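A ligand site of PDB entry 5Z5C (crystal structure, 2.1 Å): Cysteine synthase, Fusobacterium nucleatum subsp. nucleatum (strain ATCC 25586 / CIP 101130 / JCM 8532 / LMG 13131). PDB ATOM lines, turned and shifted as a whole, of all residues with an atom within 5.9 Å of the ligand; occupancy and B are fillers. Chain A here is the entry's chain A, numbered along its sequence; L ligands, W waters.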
ATOM      1  N   SER A  48       3.154  -7.898   9.601  1.00  0.00           N
ATOM      2  CA  SER A  48       2.029  -7.334  10.357  1.00  0.00           C
ATOM      3  C   SER A  48       1.607  -6.005   9.818  1.00  0.00           C
ATOM      4  O   SER A  48       2.398  -5.276   9.163  1.00  0.00           O
ATOM      5  CB  SER A  48       2.324  -7.204  11.843  1.00  0.00           C
ATOM      6  OG  SER A  48       2.769  -5.908  12.210  1.00  0.00           O
ATOM      7  N   ILE A  49       0.372  -5.679  10.138  1.00  0.00           N
ATOM      8  CA  ILE A  49      -0.232  -4.397   9.858  1.00  0.00           C
ATOM      9  C   ILE A  49       0.602  -3.226  10.389  1.00  0.00           C
ATOM     10  O   ILE A  49       0.557  -2.122   9.816  1.00  0.00           O
ATOM     11  CB  ILE A  49      -1.688  -4.367  10.388  1.00  0.00           C
ATOM     12  CG1 ILE A  49      -2.505  -3.287   9.676  1.00  0.00           C
ATOM     13  CG2 ILE A  49      -1.712  -4.281  11.922  1.00  0.00           C
ATOM     14  CD1 ILE A  49      -3.967  -3.254  10.090  1.00  0.00           C
ATOM     15  N   LYS A  50       1.392  -3.470  11.459  1.00  0.00           N
ATOM     16  CA  LYS A  50       2.157  -2.384  12.115  1.00  0.00           C
ATOM     17  C   LYS A  50       3.226  -1.834  11.263  1.00  0.00           C
ATOM     18  O   LYS A  50       3.623  -0.710  11.472  1.00  0.00           O
ATOM     19  CB  LYS A  50       2.746  -2.828  13.483  1.00  0.00           C
ATOM     20  CG  LYS A  50       1.664  -3.360  14.427  1.00  0.00           C
ATOM     21  CD  LYS A  50       0.668  -2.291  14.864  1.00  0.00           C
ATOM     22  CE  LYS A  50      -0.526  -2.919  15.527  1.00  0.00           C
ATOM     23  NZ  LYS A  50      -0.155  -3.546  16.836  1.00  0.00           N
ATOM     24  N   SER A  78       2.975  -4.253  22.300  1.00  0.00           N
ATOM     25  CA  SER A  78       2.529  -5.614  22.531  1.00  0.00           C
ATOM     26  C   SER A  78       3.315  -6.592  21.657  1.00  0.00           C
ATOM     27  O   SER A  78       3.090  -7.808  21.758  1.00  0.00           O
ATOM     28  CB  SER A  78       1.021  -5.764  22.203  1.00  0.00           C
ATOM     29  OG  SER A  78       0.817  -5.449  20.834  1.00  0.00           O
ATOM     30  N   GLY A  79       4.190  -6.089  20.783  1.00  0.00           N
ATOM     31  CA  GLY A  79       5.052  -6.973  19.978  1.00  0.00           C
ATOM     32  C   GLY A  79       5.246  -6.427  18.581  1.00  0.00           C
ATOM     33  O   GLY A  79       6.336  -6.059  18.203  1.00  0.00           O
ATOM     34  N   ASN A  80       4.138  -6.305  17.835  1.00  0.00           N
ATOM     35  CA  ASN A  80       4.258  -6.064  16.417  1.00  0.00           C
ATOM     36  C   ASN A  80       4.786  -4.687  16.073  1.00  0.00           C
ATOM     37  O   ASN A  80       5.502  -4.531  15.122  1.00  0.00           O
ATOM     38  CB  ASN A  80       2.927  -6.306  15.719  1.00  0.00           C
ATOM     39  CG  ASN A  80       2.703  -7.769  15.389  1.00  0.00           C
ATOM     40  OD1 ASN A  80       3.646  -8.474  14.990  1.00  0.00           O
ATOM     41  ND2 ASN A  80       1.449  -8.204  15.465  1.00  0.00           N
ATOM     42  N   THR A  81       4.385  -3.680  16.843  1.00  0.00           N
ATOM     43  CA  THR A  81       4.870  -2.361  16.659  1.00  0.00           C
ATOM     44  C   THR A  81       6.385  -2.292  16.944  1.00  0.00           C
ATOM     45  O   THR A  81       7.105  -1.597  16.245  1.00  0.00           O
ATOM     46  CB  THR A  81       4.095  -1.362  17.506  1.00  0.00           C
ATOM     47  OG1 THR A  81       2.820  -1.205  16.930  1.00  0.00           O
ATOM     48  CG2 THR A  81       4.672  -0.052  17.387  1.00  0.00           C
ATOM     49  N   ARG A 108       8.111 -12.884  20.101  1.00  0.00           N
ATOM     50  CA  ARG A 108       8.206 -11.416  19.930  1.00  0.00           C
ATOM     51  C   ARG A 108       9.557 -10.865  20.387  1.00  0.00           C
ATOM     52  O   ARG A 108      10.174 -10.053  19.655  1.00  0.00           O
ATOM     53  CB  ARG A 108       7.049 -10.679  20.613  1.00  0.00           C
ATOM     54  CG  ARG A 108       5.698 -10.891  19.955  1.00  0.00           C
ATOM     55  CD  ARG A 108       4.584 -10.627  20.926  1.00  0.00           C
ATOM     56  NE  ARG A 108       3.359 -10.145  20.283  1.00  0.00           N
ATOM     57  CZ  ARG A 108       2.514 -10.932  19.587  1.00  0.00           C
ATOM     58  NH1 ARG A 108       2.780 -12.221  19.412  1.00  0.00           N
ATOM     59  NH2 ARG A 108       1.427 -10.401  19.050  1.00  0.00           N
ATOM     60  N   GLN A 151       2.859   5.488  19.923  1.00  0.00           N
ATOM     61  CA  GLN A 151       1.786   4.901  19.140  1.00  0.00           C
ATOM     62  C   GLN A 151       0.426   5.014  19.825  1.00  0.00           C
ATOM     63  O   GLN A 151      -0.572   5.025  19.132  1.00  0.00           O
ATOM     64  CB  GLN A 151       2.086   3.421  18.752  1.00  0.00           C
ATOM     65  CG  GLN A 151       2.184   2.499  19.972  1.00  0.00           C
ATOM     66  CD  GLN A 151       2.176   1.013  19.645  1.00  0.00           C
ATOM     67  OE1 GLN A 151       2.688   0.185  20.457  1.00  0.00           O
ATOM     68  NE2 GLN A 151       1.491   0.631  18.538  1.00  0.00           N
ATOM     69  N   ASN A 157      -0.408   7.528  13.767  1.00  0.00           N
ATOM     70  CA  ASN A 157      -0.742   6.110  13.823  1.00  0.00           C
ATOM     71  C   ASN A 157      -2.048   5.918  13.026  1.00  0.00           C
ATOM     72  O   ASN A 157      -2.037   5.266  11.962  1.00  0.00           O
ATOM     73  CB  ASN A 157      -0.831   5.652  15.308  1.00  0.00           C
ATOM     74  CG  ASN A 157      -1.242   4.187  15.475  1.00  0.00           C
ATOM     75  OD1 ASN A 157      -1.126   3.637  16.587  1.00  0.00           O
ATOM     76  ND2 ASN A 157      -1.725   3.544  14.403  1.00  0.00           N
ATOM     77  N   HIS A 161      -3.249   4.562   8.691  1.00  0.00           N
ATOM     78  CA  HIS A 161      -4.276   3.641   8.242  1.00  0.00           C
ATOM     79  C   HIS A 161      -5.387   4.320   7.448  1.00  0.00           C
ATOM     80  O   HIS A 161      -6.028   3.710   6.589  1.00  0.00           O
ATOM     81  CB  HIS A 161      -4.836   2.885   9.420  1.00  0.00           C
ATOM     82  CG  HIS A 161      -3.824   2.092  10.151  1.00  0.00           C
ATOM     83  ND1 HIS A 161      -3.001   1.185   9.513  1.00  0.00           N
ATOM     84  CD2 HIS A 161      -3.497   2.057  11.462  1.00  0.00           C
ATOM     85  CE1 HIS A 161      -2.245   0.588  10.422  1.00  0.00           C
ATOM     86  NE2 HIS A 161      -2.499   1.106  11.602  1.00  0.00           N
ATOM     87  N   GLY A 186     -10.133  -5.130  16.484  1.00  0.00           N
ATOM     88  CA  GLY A 186      -9.603  -5.101  17.827  1.00  0.00           C
ATOM     89  C   GLY A 186      -8.771  -3.846  18.046  1.00  0.00           C
ATOM     90  O   GLY A 186      -8.047  -3.410  17.128  1.00  0.00           O
ATOM     91  N   VAL A 187      -8.910  -3.278  19.255  1.00  0.00           N
ATOM     92  CA  VAL A 187      -8.258  -2.045  19.663  1.00  0.00           C
ATOM     93  C   VAL A 187      -7.093  -2.358  20.584  1.00  0.00           C
ATOM     94  O   VAL A 187      -7.256  -2.947  21.675  1.00  0.00           O
ATOM     95  CB  VAL A 187      -9.234  -1.051  20.351  1.00  0.00           C
ATOM     96  CG1 VAL A 187      -8.490   0.127  20.955  1.00  0.00           C
ATOM     97  CG2 VAL A 187     -10.238  -0.580  19.333  1.00  0.00           C
ATOM     98  N   GLY A 188      -5.907  -2.048  20.069  1.00  0.00           N
ATOM     99  CA  GLY A 188      -4.688  -1.921  20.880  1.00  0.00           C
ATOM    100  C   GLY A 188      -4.422  -0.462  21.141  1.00  0.00           C
ATOM    101  O   GLY A 188      -4.769   0.045  22.203  1.00  0.00           O
ATOM    102  N   THR A 189      -3.811   0.215  20.175  1.00  0.00           N
ATOM    103  CA  THR A 189      -3.707   1.665  20.144  1.00  0.00           C
ATOM    104  C   THR A 189      -4.942   2.395  19.665  1.00  0.00           C
ATOM    105  O   THR A 189      -5.159   3.570  19.972  1.00  0.00           O
ATOM    106  CB  THR A 189      -2.565   2.079  19.202  1.00  0.00           C
ATOM    107  OG1 THR A 189      -2.847   1.671  17.861  1.00  0.00           O
ATOM    108  CG2 THR A 189      -1.221   1.470  19.690  1.00  0.00           C
ATOM    109  N   GLY A 190      -5.744   1.708  18.866  1.00  0.00           N
ATOM    110  CA  GLY A 190      -6.863   2.298  18.227  1.00  0.00           C
ATOM    111  C   GLY A 190      -6.568   2.832  16.852  1.00  0.00           C
ATOM    112  O   GLY A 190      -7.493   3.167  16.169  1.00  0.00           O
ATOM    113  N   GLY A 191      -5.304   2.916  16.436  1.00  0.00           N
ATOM    114  CA  GLY A 191      -4.947   3.316  15.086  1.00  0.00           C
ATOM    115  C   GLY A 191      -5.763   2.664  13.971  1.00  0.00           C
ATOM    116  O   GLY A 191      -6.252   3.361  13.095  1.00  0.00           O
ATOM    117  N   THR A 192      -5.791   1.335  13.950  1.00  0.00           N
ATOM    118  CA  THR A 192      -6.462   0.577  12.911  1.00  0.00           C
ATOM    119  C   THR A 192      -7.911   1.026  12.797  1.00  0.00           C
ATOM    120  O   THR A 192      -8.333   1.510  11.766  1.00  0.00           O
ATOM    121  CB  THR A 192      -6.369  -0.927  13.215  1.00  0.00           C
ATOM    122  OG1 THR A 192      -4.972  -1.303  13.226  1.00  0.00           O
ATOM    123  CG2 THR A 192      -7.145  -1.784  12.148  1.00  0.00           C
ATOM    124  N   VAL A 193      -8.658   0.932  13.884  1.00  0.00           N
ATOM    125  CA  VAL A 193     -10.106   1.235  13.812  1.00  0.00           C
ATOM    126  C   VAL A 193     -10.413   2.693  13.547  1.00  0.00           C
ATOM    127  O   VAL A 193     -11.372   2.997  12.823  1.00  0.00           O
ATOM    128  CB  VAL A 193     -10.927   0.729  15.034  1.00  0.00           C
ATOM    129  CG1 VAL A 193     -10.795   1.596  16.282  1.00  0.00           C
ATOM    130  CG2 VAL A 193     -12.382   0.563  14.668  1.00  0.00           C
ATOM    131  N   GLU A 232      -3.371 -11.289  21.954  1.00  0.00           N
ATOM    132  CA  GLU A 232      -2.177 -10.488  21.873  1.00  0.00           C
ATOM    133  C   GLU A 232      -2.366  -9.401  20.834  1.00  0.00           C
ATOM    134  O   GLU A 232      -2.852  -9.675  19.700  1.00  0.00           O
ATOM    135  CB  GLU A 232      -0.916 -11.350  21.608  1.00  0.00           C
ATOM    136  CG  GLU A 232      -0.711 -12.448  22.669  1.00  0.00           C
ATOM    137  CD  GLU A 232       0.637 -13.134  22.701  1.00  0.00           C
ATOM    138  OE1 GLU A 232       1.667 -12.482  22.420  1.00  0.00           O
ATOM    139  OE2 GLU A 232       0.666 -14.311  23.116  1.00  0.00           O
ATOM    140  N   GLY A 233      -2.002  -8.167  21.222  1.00  0.00           N
ATOM    141  CA  GLY A 233      -2.075  -6.989  20.341  1.00  0.00           C
ATOM    142  C   GLY A 233      -3.184  -6.021  20.694  1.00  0.00           C
ATOM    143  O   GLY A 233      -3.100  -4.856  20.335  1.00  0.00           O
ATOM    144  N   ILE A 234      -4.231  -6.500  21.386  1.00  0.00           N
ATOM    145  CA  ILE A 234      -5.353  -5.675  21.759  1.00  0.00           C
ATOM    146  C   ILE A 234      -5.502  -5.587  23.278  1.00  0.00           C
ATOM    147  O   ILE A 234      -5.016  -6.449  24.004  1.00  0.00           O
ATOM    148  CB  ILE A 234      -6.689  -6.130  21.102  1.00  0.00           C
ATOM    149  CG1 ILE A 234      -7.246  -7.401  21.726  1.00  0.00           C
ATOM    150  CG2 ILE A 234      -6.485  -6.334  19.608  1.00  0.00           C
ATOM    151  CD1 ILE A 234      -8.682  -7.645  21.300  1.00  0.00           C
ATOM    152  N   SER A 276      -5.570 -12.426  17.450  1.00  0.00           N
ATOM    153  CA  SER A 276      -6.428 -11.254  17.181  1.00  0.00           C
ATOM    154  C   SER A 276      -7.155 -11.328  15.839  1.00  0.00           C
ATOM    155  O   SER A 276      -8.266 -10.741  15.678  1.00  0.00           O
ATOM    156  CB  SER A 276      -5.628  -9.918  17.301  1.00  0.00           C
ATOM    157  OG  SER A 276      -4.868  -9.680  16.121  1.00  0.00           O
ATOM    158  N   SER A 277      -6.616 -12.089  14.892  1.00  0.00           N
ATOM    159  CA  SER A 277      -7.311 -12.306  13.602  1.00  0.00           C
ATOM    160  C   SER A 277      -8.568 -13.161  13.779  1.00  0.00           C
ATOM    161  O   SER A 277      -9.614 -12.882  13.199  1.00  0.00           O
ATOM    162  CB  SER A 277      -6.392 -12.990  12.594  1.00  0.00           C
ATOM    163  OG  SER A 277      -5.305 -12.130  12.245  1.00  0.00           O
ATOM    164  N   ASN A 280     -11.075 -10.824  15.488  1.00  0.00           N
ATOM    165  CA  ASN A 280     -11.688  -9.970  14.457  1.00  0.00           C
ATOM    166  C   ASN A 280     -12.719 -10.688  13.550  1.00  0.00           C
ATOM    167  O   ASN A 280     -13.710 -10.097  13.166  1.00  0.00           O
ATOM    168  CB  ASN A 280     -10.621  -9.348  13.577  1.00  0.00           C
ATOM    169  CG  ASN A 280      -9.913  -8.192  14.276  1.00  0.00           C
ATOM    170  OD1 ASN A 280     -10.297  -7.835  15.377  1.00  0.00           O
ATOM    171  ND2 ASN A 280      -8.960  -7.573  13.611  1.00  0.00           N
ATOM    172  N   PRO A 302      -4.364  -9.007  11.427  1.00  0.00           N
ATOM    173  CA  PRO A 302      -3.123  -8.222  11.627  1.00  0.00           C
ATOM    174  C   PRO A 302      -1.810  -8.939  11.394  1.00  0.00           C
ATOM    175  O   PRO A 302      -0.872  -8.291  10.971  1.00  0.00           O
ATOM    176  CB  PRO A 302      -3.200  -7.820  13.093  1.00  0.00           C
ATOM    177  CG  PRO A 302      -4.686  -7.595  13.256  1.00  0.00           C
ATOM    178  CD  PRO A 302      -5.263  -8.826  12.579  1.00  0.00           C
ATOM    179  N   ASP A 303      -1.735 -10.252  11.648  1.00  0.00           N
ATOM    180  CA  ASP A 303      -0.474 -10.972  11.464  1.00  0.00           C
ATOM    181  C   ASP A 303      -0.738 -12.455  11.251  1.00  0.00           C
ATOM    182  O   ASP A 303      -1.899 -12.890  11.295  1.00  0.00           O
ATOM    183  CB  ASP A 303       0.509 -10.693  12.611  1.00  0.00           C
ATOM    184  CG  ASP A 303       0.054 -11.220  13.959  1.00  0.00           C
ATOM    185  OD1 ASP A 303      -1.039 -11.795  14.044  1.00  0.00           O
ATOM    186  OD2 ASP A 303       0.781 -11.060  14.916  1.00  0.00           O
ATOM    187  N   TYR A 308       3.142 -17.432  17.276  1.00  0.00           N
ATOM    188  CA  TYR A 308       2.225 -17.964  18.290  1.00  0.00           C
ATOM    189  C   TYR A 308       2.376 -19.425  18.579  1.00  0.00           C
ATOM    190  O   TYR A 308       1.601 -19.958  19.346  1.00  0.00           O
ATOM    191  CB  TYR A 308       0.752 -17.640  17.905  1.00  0.00           C
ATOM    192  CG  TYR A 308       0.496 -16.191  17.738  1.00  0.00           C
ATOM    193  CD1 TYR A 308       0.688 -15.579  16.510  1.00  0.00           C
ATOM    194  CD2 TYR A 308       0.076 -15.409  18.798  1.00  0.00           C
ATOM    195  CE1 TYR A 308       0.463 -14.237  16.338  1.00  0.00           C
ATOM    196  CE2 TYR A 308      -0.156 -14.058  18.647  1.00  0.00           C
ATOM    197  CZ  TYR A 308       0.038 -13.479  17.404  1.00  0.00           C
ATOM    198  OH  TYR A 308      -0.175 -12.135  17.216  1.00  0.00           O
HETATM  199  N1  LIG L   1      -3.632  -7.335  16.598  1.00  0.00           N
HETATM  200  C1  LIG L   1      -2.293  -7.443  16.594  1.00  0.00           C
HETATM  201  C2  LIG L   1      -1.612  -8.751  16.343  1.00  0.00           C
HETATM  202  C3  LIG L   1      -1.458  -6.249  16.831  1.00  0.00           C
HETATM  203  O1  LIG L   1      -0.112  -6.272  16.869  1.00  0.00           O
HETATM  204  C4  LIG L   1      -2.165  -4.995  17.081  1.00  0.00           C
HETATM  205  C5  LIG L   1      -1.354  -3.808  17.336  1.00  0.00           C
HETATM  206  C6  LIG L   1      -3.641  -4.998  17.069  1.00  0.00           C
HETATM  207  C7  LIG L   1      -4.294  -6.198  16.814  1.00  0.00           C
HETATM  208  C8  LIG L   1      -4.399  -3.709  17.325  1.00  0.00           C
HETATM  209  O2  LIG L   1      -4.150  -2.676  16.358  1.00  0.00           O
HETATM  210  P1  LIG L   1      -4.215  -1.129  16.789  1.00  0.00           P
HETATM  211  O3  LIG L   1      -5.522  -0.957  17.508  1.00  0.00           O
HETATM  212  O4  LIG L   1      -3.051  -0.850  17.744  1.00  0.00           O
HETATM  213  O5  LIG L   1      -4.020  -0.394  15.494  1.00  0.00           O
HETATM  214  O   HOH W   1       1.421  -7.324  18.933  1.00  0.00           O
HETATM  215  O   HOH W   2      -7.787  -0.628  16.279  1.00  0.00           O
HETATM  216  O   HOH W   3      -1.803   0.729  14.386  1.00  0.00           O
HETATM  217  O   HOH W   4      -4.906  -3.993  13.814  1.00  0.00           O
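OG1 of Thr 192 lies within hydrogen-bond range of O5 of the ligand (2.6 Å).
The backbone NH (N) of Gly 188 lies within hydrogen-bond range of an oxygen (O3) of the ligand, 2.8 Å away.
N1 of the ligand sits at hydrogen-bond distance from OG of Ser 276, 2.7 Å away.
C5 of the ligand is bonded to NZ of Lys 50 (1.3 Å).
The backbone NH (N) of Gly 190 sits at hydrogen-bond distance from an oxygen (O3) of the ligand (3.0 Å).
An oxygen (O4) of the ligand lies within hydrogen-bond range of the backbone NH (N) of Thr 189.
N of Thr 192 lies within hydrogen-bond range of O5 of the ligand, 2.9 Å away.
O4 of the ligand lies within hydrogen-bond range of OG1 of Thr 189 (2.5 Å).
The side-chain amide nitrogen (ND2) of Asn 80 is in hydrogen-bond range of an oxygen (O1) of the ligand, at 2.9 Å.
O of Pro 302 lies within hydrogen-bond range of N of Ile 49 (3.0 Å).
The side-chain amide nitrogen (ND2) of Asn 80 is in hydrogen-bond range of the side-chain carboxylate (OD2) of Asp 303 (3.0 Å).
The side-chain carboxylate (OE1) of Glu 232 is in salt-bridge range of the guanidinium group (NH1) of Arg 108 (3.2 Å).
OG1 of Thr 189 is in hydrogen-bond range of OD1 of Asn 157, 2.9 Å away.
OH of Tyr 308 lies within hydrogen-bond range of NH2 of Arg 108 (3.0 Å).
N of Lys 50 is in hydrogen-bond range of OG of Ser 48.
OD2 of Asp 303 is in hydrogen-bond range of OH of Tyr 308, 2.7 Å away.
The side-chain hydroxyl (OG1) of Thr 189 lies within hydrogen-bond range of the backbone NH (N) of Gly 191.
Merely in contact with the ligand: Gly 186 (3.5 Å), Val 187 (3.6 Å), Gly 191 (3.7 Å), Glu 232 (3.7 Å), Gly 233 (3.3 Å), Ile 234 (3.6 Å), Pro 302 (3.5 Å), Asp 303 (3.6 Å) and Tyr 308 (3.8 Å).
Hydrophobic or aromatic side chains within 4 Å of the ligand: Ile 234 and Pro 302.
Within 4 Å of the ligand: Lys 50, Asn 80, Gly 186, Val 187, Gly 188, Thr 189, Gly 190, Gly 191, Thr 192, Glu 232, Gly 233, Ile 234, Ser 276, Pro 302, Asp 303 and Tyr 308.
Water W2 lies within hydrogen-bond range of an oxygen (O3) of the ligand (2.6 Å), the backbone carbonyl oxygen of Gly 186 (2.9 Å) and the backbone NH of Val 193 (3.0 Å).
Water W3 lies within hydrogen-bond range of an oxygen (O5) of the ligand, the side-chain amide nitrogen (ND2) of Asn 157 and a ring nitrogen (NE2) of His 161.
Water W1 lies within hydrogen-bond range of the side-chain hydroxyl (OG) of Ser 78 (2.7 Å), an oxygen (O1) of the ligand (2.8 Å), the guanidinium group (NH2) of Arg 108 (3.1 Å) and the backbone NH (N) of Asn 80 (3.1 Å).
Water W4 bridges OG1 of Thr 192 and O2 of the ligand.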
